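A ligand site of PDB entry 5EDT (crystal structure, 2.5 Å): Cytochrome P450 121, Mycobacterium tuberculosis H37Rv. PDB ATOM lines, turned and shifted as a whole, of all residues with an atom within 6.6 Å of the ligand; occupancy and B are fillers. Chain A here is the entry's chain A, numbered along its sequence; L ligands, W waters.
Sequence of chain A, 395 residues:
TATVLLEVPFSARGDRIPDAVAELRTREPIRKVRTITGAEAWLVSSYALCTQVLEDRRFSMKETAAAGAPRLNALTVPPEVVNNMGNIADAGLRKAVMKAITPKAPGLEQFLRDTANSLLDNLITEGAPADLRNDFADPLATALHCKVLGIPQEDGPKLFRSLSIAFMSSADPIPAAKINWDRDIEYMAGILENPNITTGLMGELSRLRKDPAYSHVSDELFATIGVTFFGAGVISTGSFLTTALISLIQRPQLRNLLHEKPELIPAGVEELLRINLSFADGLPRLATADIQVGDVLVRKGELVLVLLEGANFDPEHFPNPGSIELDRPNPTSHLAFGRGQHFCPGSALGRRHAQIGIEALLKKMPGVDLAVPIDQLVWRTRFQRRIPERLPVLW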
ATOM      1  N   THR A  76      12.243  -5.808  -3.792  1.00  0.00           N
ATOM      2  CA  THR A  76      11.083  -6.587  -4.239  1.00  0.00           C
ATOM      3  C   THR A  76      11.239  -6.949  -5.712  1.00  0.00           C
ATOM      4  O   THR A  76      10.352  -7.516  -6.303  1.00  0.00           O
ATOM      5  CB  THR A  76       9.751  -5.842  -3.938  1.00  0.00           C
ATOM      6  OG1 THR A  76       9.529  -4.765  -4.865  1.00  0.00           O
ATOM      7  CG2 THR A  76       9.757  -5.279  -2.491  1.00  0.00           C
ATOM      8  N   VAL A  77      12.409  -6.615  -6.272  1.00  0.00           N
ATOM      9  CA  VAL A  77      12.799  -6.887  -7.654  1.00  0.00           C
ATOM     10  C   VAL A  77      14.221  -7.447  -7.733  1.00  0.00           C
ATOM     11  O   VAL A  77      15.018  -7.253  -6.808  1.00  0.00           O
ATOM     12  CB  VAL A  77      12.703  -5.642  -8.510  1.00  0.00           C
ATOM     13  CG1 VAL A  77      11.268  -5.171  -8.578  1.00  0.00           C
ATOM     14  CG2 VAL A  77      13.563  -4.516  -7.943  1.00  0.00           C
ATOM     15  N   VAL A  81      17.043  -4.621 -11.876  1.00  0.00           N
ATOM     16  CA  VAL A  81      15.810  -3.876 -12.211  1.00  0.00           C
ATOM     17  C   VAL A  81      15.763  -2.489 -11.530  1.00  0.00           C
ATOM     18  O   VAL A  81      15.082  -1.583 -11.978  1.00  0.00           O
ATOM     19  CB  VAL A  81      14.534  -4.750 -11.955  1.00  0.00           C
ATOM     20  CG1 VAL A  81      13.215  -3.982 -12.170  1.00  0.00           C
ATOM     21  CG2 VAL A  81      14.537  -6.012 -12.825  1.00  0.00           C
ATOM     22  N   LEU A 159      -3.180  -8.735 -12.571  1.00  0.00           N
ATOM     23  CA  LEU A 159      -1.943  -8.009 -12.476  1.00  0.00           C
ATOM     24  C   LEU A 159      -1.932  -6.972 -11.327  1.00  0.00           C
ATOM     25  O   LEU A 159      -0.904  -6.787 -10.671  1.00  0.00           O
ATOM     26  CB  LEU A 159      -1.540  -7.390 -13.806  1.00  0.00           C
ATOM     27  CG  LEU A 159      -1.221  -8.363 -14.939  1.00  0.00           C
ATOM     28  CD1 LEU A 159      -1.187  -7.557 -16.230  1.00  0.00           C
ATOM     29  CD2 LEU A 159       0.112  -9.039 -14.695  1.00  0.00           C
ATOM     30  N   SER A 162      -0.991  -8.133  -7.646  1.00  0.00           N
ATOM     31  CA  SER A 162       0.385  -8.259  -7.256  1.00  0.00           C
ATOM     32  C   SER A 162       0.869  -7.011  -6.470  1.00  0.00           C
ATOM     33  O   SER A 162       1.874  -7.100  -5.735  1.00  0.00           O
ATOM     34  CB  SER A 162       1.272  -8.387  -8.495  1.00  0.00           C
ATOM     35  OG  SER A 162       1.167  -9.670  -9.086  1.00  0.00           O
ATOM     36  N   LEU A 163       0.186  -5.864  -6.639  1.00  0.00           N
ATOM     37  CA  LEU A 163       0.725  -4.577  -6.179  1.00  0.00           C
ATOM     38  C   LEU A 163       0.756  -4.321  -4.674  1.00  0.00           C
ATOM     39  O   LEU A 163       1.643  -3.592  -4.188  1.00  0.00           O
ATOM     40  CB  LEU A 163       0.091  -3.434  -6.937  1.00  0.00           C
ATOM     41  CG  LEU A 163       0.291  -3.538  -8.455  1.00  0.00           C
ATOM     42  CD1 LEU A 163      -0.258  -2.251  -9.088  1.00  0.00           C
ATOM     43  CD2 LEU A 163       1.754  -3.734  -8.862  1.00  0.00           C
ATOM     44  N   ILE A 165       1.652  -6.411  -2.582  1.00  0.00           N
ATOM     45  CA  ILE A 165       2.933  -7.029  -2.230  1.00  0.00           C
ATOM     46  C   ILE A 165       4.135  -6.348  -2.932  1.00  0.00           C
ATOM     47  O   ILE A 165       5.141  -6.054  -2.263  1.00  0.00           O
ATOM     48  CB  ILE A 165       2.920  -8.539  -2.503  1.00  0.00           C
ATOM     49  CG1 ILE A 165       2.148  -9.242  -1.370  1.00  0.00           C
ATOM     50  CG2 ILE A 165       4.342  -9.090  -2.517  1.00  0.00           C
ATOM     51  CD1 ILE A 165       1.220 -10.309  -1.861  1.00  0.00           C
ATOM     52  N   ALA A 166       4.006  -6.025  -4.214  1.00  0.00           N
ATOM     53  CA  ALA A 166       5.131  -5.525  -4.997  1.00  0.00           C
ATOM     54  C   ALA A 166       5.704  -4.261  -4.451  1.00  0.00           C
ATOM     55  O   ALA A 166       6.912  -4.028  -4.591  1.00  0.00           O
ATOM     56  CB  ALA A 166       4.725  -5.284  -6.414  1.00  0.00           C
ATOM     57  N   PHE A 167       4.835  -3.434  -3.856  1.00  0.00           N
ATOM     58  CA  PHE A 167       5.253  -2.119  -3.349  1.00  0.00           C
ATOM     59  C   PHE A 167       5.318  -2.047  -1.846  1.00  0.00           C
ATOM     60  O   PHE A 167       5.272  -0.938  -1.251  1.00  0.00           O
ATOM     61  CB  PHE A 167       4.432  -1.024  -3.994  1.00  0.00           C
ATOM     62  CG  PHE A 167       4.818  -0.805  -5.421  1.00  0.00           C
ATOM     63  CD1 PHE A 167       4.287  -1.594  -6.430  1.00  0.00           C
ATOM     64  CD2 PHE A 167       5.806   0.134  -5.757  1.00  0.00           C
ATOM     65  CE1 PHE A 167       4.708  -1.420  -7.750  1.00  0.00           C
ATOM     66  CE2 PHE A 167       6.225   0.313  -7.060  1.00  0.00           C
ATOM     67  CZ  PHE A 167       5.686  -0.473  -8.065  1.00  0.00           C
ATOM     68  N   ALA A 176       6.528 -13.631  -1.473  1.00  0.00           N
ATOM     69  CA  ALA A 176       5.414 -13.487  -2.374  1.00  0.00           C
ATOM     70  C   ALA A 176       5.740 -12.578  -3.568  1.00  0.00           C
ATOM     71  O   ALA A 176       5.171 -12.784  -4.642  1.00  0.00           O
ATOM     72  CB  ALA A 176       4.154 -13.027  -1.629  1.00  0.00           C
ATOM     73  N   ALA A 177       6.652 -11.612  -3.388  1.00  0.00           N
ATOM     74  CA  ALA A 177       7.044 -10.665  -4.454  1.00  0.00           C
ATOM     75  C   ALA A 177       7.723 -11.381  -5.616  1.00  0.00           C
ATOM     76  O   ALA A 177       7.489 -11.048  -6.805  1.00  0.00           O
ATOM     77  CB  ALA A 177       7.926  -9.563  -3.919  1.00  0.00           C
ATOM     78  N   LYS A 178       8.545 -12.388  -5.278  1.00  0.00           N
ATOM     79  CA  LYS A 178       9.230 -13.188  -6.265  1.00  0.00           C
ATOM     80  C   LYS A 178       8.226 -14.036  -7.106  1.00  0.00           C
ATOM     81  O   LYS A 178       8.239 -13.976  -8.369  1.00  0.00           O
ATOM     82  CB  LYS A 178      10.244 -14.093  -5.553  1.00  0.00           C
ATOM     83  CG  LYS A 178      10.763 -15.202  -6.436  1.00  0.00           C
ATOM     84  CD  LYS A 178      12.230 -15.503  -6.176  1.00  0.00           C
ATOM     85  CE  LYS A 178      12.601 -16.809  -6.866  1.00  0.00           C
ATOM     86  NZ  LYS A 178      12.526 -16.830  -8.384  1.00  0.00           N
ATOM     87  N   ILE A 179       7.403 -14.820  -6.418  1.00  0.00           N
ATOM     88  CA  ILE A 179       6.276 -15.478  -7.039  1.00  0.00           C
ATOM     89  C   ILE A 179       5.510 -14.570  -8.041  1.00  0.00           C
ATOM     90  O   ILE A 179       5.390 -14.920  -9.245  1.00  0.00           O
ATOM     91  CB  ILE A 179       5.294 -16.010  -5.965  1.00  0.00           C
ATOM     92  CG1 ILE A 179       6.069 -16.902  -4.956  1.00  0.00           C
ATOM     93  CG2 ILE A 179       4.099 -16.693  -6.632  1.00  0.00           C
ATOM     94  CD1 ILE A 179       5.232 -17.600  -3.912  1.00  0.00           C
ATOM     95  N   ASN A 180       5.013 -13.425  -7.573  1.00  0.00           N
ATOM     96  CA  ASN A 180       4.249 -12.524  -8.424  1.00  0.00           C
ATOM     97  C   ASN A 180       5.117 -12.013  -9.543  1.00  0.00           C
ATOM     98  O   ASN A 180       4.712 -12.050 -10.686  1.00  0.00           O
ATOM     99  CB  ASN A 180       3.688 -11.347  -7.633  1.00  0.00           C
ATOM    100  CG  ASN A 180       2.504 -11.729  -6.751  1.00  0.00           C
ATOM    101  OD1 ASN A 180       1.749 -12.688  -7.051  1.00  0.00           O
ATOM    102  ND2 ASN A 180       2.293 -10.948  -5.679  1.00  0.00           N
ATOM    103  N   TRP A 181       6.305 -11.528  -9.211  1.00  0.00           N
ATOM    104  CA  TRP A 181       7.231 -11.043 -10.240  1.00  0.00           C
ATOM    105  C   TRP A 181       7.452 -12.012 -11.357  1.00  0.00           C
ATOM    106  O   TRP A 181       7.281 -11.689 -12.556  1.00  0.00           O
ATOM    107  CB  TRP A 181       8.569 -10.741  -9.602  1.00  0.00           C
ATOM    108  CG  TRP A 181       9.581 -10.287 -10.600  1.00  0.00           C
ATOM    109  CD1 TRP A 181      10.618 -11.038 -11.203  1.00  0.00           C
ATOM    110  CD2 TRP A 181       9.714  -8.953 -11.160  1.00  0.00           C
ATOM    111  NE1 TRP A 181      11.341 -10.262 -12.039  1.00  0.00           N
ATOM    112  CE2 TRP A 181      10.850  -9.003 -12.079  1.00  0.00           C
ATOM    113  CE3 TRP A 181       9.027  -7.747 -10.980  1.00  0.00           C
ATOM    114  CZ2 TRP A 181      11.263  -7.895 -12.777  1.00  0.00           C
ATOM    115  CZ3 TRP A 181       9.458  -6.628 -11.699  1.00  0.00           C
ATOM    116  CH2 TRP A 181      10.538  -6.709 -12.586  1.00  0.00           C
ATOM    117  N   ASP A 182       7.841 -13.234 -10.981  1.00  0.00           N
ATOM    118  CA  ASP A 182       8.088 -14.306 -11.964  1.00  0.00           C
ATOM    119  C   ASP A 182       6.830 -14.605 -12.776  1.00  0.00           C
ATOM    120  O   ASP A 182       6.909 -14.753 -14.002  1.00  0.00           O
ATOM    121  CB  ASP A 182       8.618 -15.599 -11.318  1.00  0.00           C
ATOM    122  CG  ASP A 182      10.057 -15.446 -10.738  1.00  0.00           C
ATOM    123  OD1 ASP A 182      10.841 -14.507 -11.129  1.00  0.00           O
ATOM    124  OD2 ASP A 182      10.399 -16.314  -9.880  1.00  0.00           O
ATOM    125  N   ARG A 183       5.692 -14.643 -12.103  1.00  0.00           N
ATOM    126  CA  ARG A 183       4.431 -14.915 -12.778  1.00  0.00           C
ATOM    127  C   ARG A 183       4.089 -13.801 -13.785  1.00  0.00           C
ATOM    128  O   ARG A 183       3.800 -14.073 -14.958  1.00  0.00           O
ATOM    129  CB  ARG A 183       3.279 -15.179 -11.784  1.00  0.00           C
ATOM    130  CG  ARG A 183       2.084 -15.928 -12.444  1.00  0.00           C
ATOM    131  CD  ARG A 183       0.798 -15.950 -11.603  1.00  0.00           C
ATOM    132  NE  ARG A 183       0.537 -14.550 -11.268  1.00  0.00           N
ATOM    133  CZ  ARG A 183       0.745 -13.993 -10.055  1.00  0.00           C
ATOM    134  NH1 ARG A 183       1.132 -14.747  -8.984  1.00  0.00           N
ATOM    135  NH2 ARG A 183       0.577 -12.672  -9.924  1.00  0.00           N
ATOM    136  N   ASP A 184       4.132 -12.556 -13.333  1.00  0.00           N
ATOM    137  CA  ASP A 184       3.821 -11.402 -14.167  1.00  0.00           C
ATOM    138  C   ASP A 184       4.834 -11.208 -15.289  1.00  0.00           C
ATOM    139  O   ASP A 184       4.453 -10.708 -16.337  1.00  0.00           O
ATOM    140  CB  ASP A 184       3.721 -10.144 -13.323  1.00  0.00           C
ATOM    141  CG  ASP A 184       2.610 -10.224 -12.347  1.00  0.00           C
ATOM    142  OD1 ASP A 184       1.706 -11.101 -12.511  1.00  0.00           O
ATOM    143  OD2 ASP A 184       2.602  -9.420 -11.408  1.00  0.00           O
ATOM    144  N   ILE A 185       6.091 -11.619 -15.079  1.00  0.00           N
ATOM    145  CA  ILE A 185       7.076 -11.648 -16.174  1.00  0.00           C
ATOM    146  C   ILE A 185       6.678 -12.723 -17.236  1.00  0.00           C
ATOM    147  O   ILE A 185       6.718 -12.426 -18.443  1.00  0.00           O
ATOM    148  CB  ILE A 185       8.544 -11.873 -15.664  1.00  0.00           C
ATOM    149  CG1 ILE A 185       9.115 -10.645 -14.924  1.00  0.00           C
ATOM    150  CG2 ILE A 185       9.469 -12.337 -16.771  1.00  0.00           C
ATOM    151  CD1 ILE A 185       9.479  -9.456 -15.788  1.00  0.00           C
ATOM    152  N   VAL A 227       6.038  -5.263 -16.931  1.00  0.00           N
ATOM    153  CA  VAL A 227       5.715  -5.491 -15.513  1.00  0.00           C
ATOM    154  C   VAL A 227       5.985  -4.206 -14.711  1.00  0.00           C
ATOM    155  O   VAL A 227       5.117  -3.751 -13.936  1.00  0.00           O
ATOM    156  CB  VAL A 227       6.527  -6.669 -14.869  1.00  0.00           C
ATOM    157  CG1 VAL A 227       6.251  -6.739 -13.366  1.00  0.00           C
ATOM    158  CG2 VAL A 227       6.240  -8.001 -15.576  1.00  0.00           C
ATOM    159  N   THR A 228       7.185  -3.648 -14.889  1.00  0.00           N
ATOM    160  CA  THR A 228       7.549  -2.431 -14.176  1.00  0.00           C
ATOM    161  C   THR A 228       6.676  -1.208 -14.501  1.00  0.00           C
ATOM    162  O   THR A 228       6.375  -0.385 -13.620  1.00  0.00           O
ATOM    163  CB  THR A 228       9.036  -2.090 -14.296  1.00  0.00           C
ATOM    164  OG1 THR A 228       9.363  -1.957 -15.676  1.00  0.00           O
ATOM    165  CG2 THR A 228       9.898  -3.196 -13.656  1.00  0.00           C
ATOM    166  N   PHE A 229       6.266  -1.067 -15.750  1.00  0.00           N
ATOM    167  CA  PHE A 229       5.569   0.142 -16.093  1.00  0.00           C
ATOM    168  C   PHE A 229       4.150  -0.032 -15.708  1.00  0.00           C
ATOM    169  O   PHE A 229       3.547   0.901 -15.212  1.00  0.00           O
ATOM    170  CB  PHE A 229       5.774   0.579 -17.557  1.00  0.00           C
ATOM    171  CG  PHE A 229       6.998   1.481 -17.747  1.00  0.00           C
ATOM    172  CD1 PHE A 229       8.309   1.004 -17.495  1.00  0.00           C
ATOM    173  CD2 PHE A 229       6.857   2.829 -18.157  1.00  0.00           C
ATOM    174  CE1 PHE A 229       9.423   1.814 -17.665  1.00  0.00           C
ATOM    175  CE2 PHE A 229       7.980   3.637 -18.306  1.00  0.00           C
ATOM    176  CZ  PHE A 229       9.264   3.126 -18.081  1.00  0.00           C
ATOM    177  N   PHE A 230       3.619  -1.232 -15.841  1.00  0.00           N
ATOM    178  CA  PHE A 230       2.294  -1.526 -15.265  1.00  0.00           C
ATOM    179  C   PHE A 230       2.279  -1.219 -13.753  1.00  0.00           C
ATOM    180  O   PHE A 230       1.457  -0.392 -13.279  1.00  0.00           O
ATOM    181  CB  PHE A 230       1.807  -2.960 -15.528  1.00  0.00           C
ATOM    182  CG  PHE A 230       0.435  -3.204 -14.970  1.00  0.00           C
ATOM    183  CD1 PHE A 230       0.274  -3.637 -13.659  1.00  0.00           C
ATOM    184  CD2 PHE A 230      -0.703  -2.930 -15.737  1.00  0.00           C
ATOM    185  CE1 PHE A 230      -0.975  -3.827 -13.111  1.00  0.00           C
ATOM    186  CE2 PHE A 230      -1.963  -3.111 -15.194  1.00  0.00           C
ATOM    187  CZ  PHE A 230      -2.112  -3.577 -13.881  1.00  0.00           C
ATOM    188  N   GLY A 231       3.196  -1.838 -13.010  1.00  0.00           N
ATOM    189  CA  GLY A 231       3.201  -1.752 -11.566  1.00  0.00           C
ATOM    190  C   GLY A 231       3.455  -0.364 -10.996  1.00  0.00           C
ATOM    191  O   GLY A 231       2.677   0.100 -10.143  1.00  0.00           O
ATOM    192  N   ALA A 232       4.558   0.293 -11.425  1.00  0.00           N
ATOM    193  CA  ALA A 232       4.881   1.639 -10.995  1.00  0.00           C
ATOM    194  C   ALA A 232       3.737   2.605 -11.301  1.00  0.00           C
ATOM    195  O   ALA A 232       3.376   3.401 -10.446  1.00  0.00           O
ATOM    196  CB  ALA A 232       6.151   2.125 -11.666  1.00  0.00           C
HETATM  197  N1  LIG L   1       7.345  -7.867  -7.327  1.00  0.00           N
HETATM  198  C1  LIG L   1       7.199  -6.718  -8.015  1.00  0.00           C
HETATM  199  C2  LIG L   1       8.078  -5.646  -7.772  1.00  0.00           C
HETATM  200  C3  LIG L   1       7.931  -4.457  -8.519  1.00  0.00           C
HETATM  201  C4  LIG L   1       6.927  -4.356  -9.475  1.00  0.00           C
HETATM  202 CL1  LIG L   1       6.605  -2.915 -10.370  1.00  0.00          CL
HETATM  203  C5  LIG L   1       6.047  -5.423  -9.701  1.00  0.00           C
HETATM  204  C6  LIG L   1       6.158  -6.644  -9.001  1.00  0.00           C
HETATM  205  C7  LIG L   1       5.224  -7.694  -9.300  1.00  0.00           C
HETATM  206  O1  LIG L   1       5.117  -8.640  -8.544  1.00  0.00           O
HETATM  207  N2  LIG L   1       4.384  -7.559 -10.336  1.00  0.00           N
HETATM  208  O   HOH W   1       4.223  -8.734  -5.832  1.00  0.00           O
HETATM  209  O   HOH W   2       3.479  -5.063 -11.721  1.00  0.00           O
HETATM  210  O   HOH W   3       1.574  -6.914 -11.928  1.00  0.00           O
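A nitrogen (N1) of the ligand is in hydrogen-bond range of the backbone carbonyl oxygen of Ala 177, at 3.2 Å. N of Trp 181 is in hydrogen-bond range of O1 of the ligand. N2 of the ligand lies within hydrogen-bond range of OD2 of Asp 184 (2.8 Å). The backbone carbonyl oxygen of Thr 76 sits at hydrogen-bond distance from a nitrogen (N1) of the ligand, at 3.2 Å.
OD2 of Asp 184 lies within hydrogen-bond range of OG of Ser 162, 2.7 Å away. The side-chain carboxylate (OD1) of Asp 184 is in salt-bridge range of the guanidinium group (NH2) of Arg 183 (3.2 Å). The side-chain hydroxyl (OG1) of Thr 76 is in hydrogen-bond range of the backbone carbonyl oxygen (O) of Ala 166. The side-chain hydroxyl (OG) of Ser 162 is in hydrogen-bond range of the guanidinium group (NH2) of Arg 183 (3.2 Å). OD1 of Asn 180 is in hydrogen-bond range of NH1 of Arg 183, at 2.9 Å.
Val 77 touches the ligand. Ser 162 touches the ligand. CB of Ala 166 touches C6 of the ligand, at 3.3 Å. CZ of Phe 167 touches CL1 of the ligand, 3.5 Å away. Asn 180 touches the ligand. CG1 of Val 227 touches N2 of the ligand (3.7 Å). Thr 228 touches the ligand (CA to CL1, 3.95 Å). Gly 231 touches the ligand. N of Ala 232 touches CL1 of the ligand, 3.9 Å away. Of the 25 residues printed, 13 come within 4 Å of the ligand. Along chain A the residues within 4 Å of the ligand span positions 76 to 232. The nearest printed residue that does not touch the ligand is Leu 163 (4.7 Å).
Water W1 lies within hydrogen-bond range of an oxygen (O1) of the ligand (2.9 Å), the backbone carbonyl oxygen of Ser 162 (2.9 Å), the side-chain amide nitrogen of Asn 180 (2.9 Å) and the backbone NH of Ala 166 (3.2 Å). Water W2 lies within hydrogen-bond range of N2 of the ligand (3.0 Å), O of Val 227 (3.1 Å) and N of Gly 231 (3.5 Å). Water W3 lies within hydrogen-bond range of OD2 of Asp 184 (2.8 Å), O of Leu 159 (2.8 Å) and N2 of the ligand (3.3 Å).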
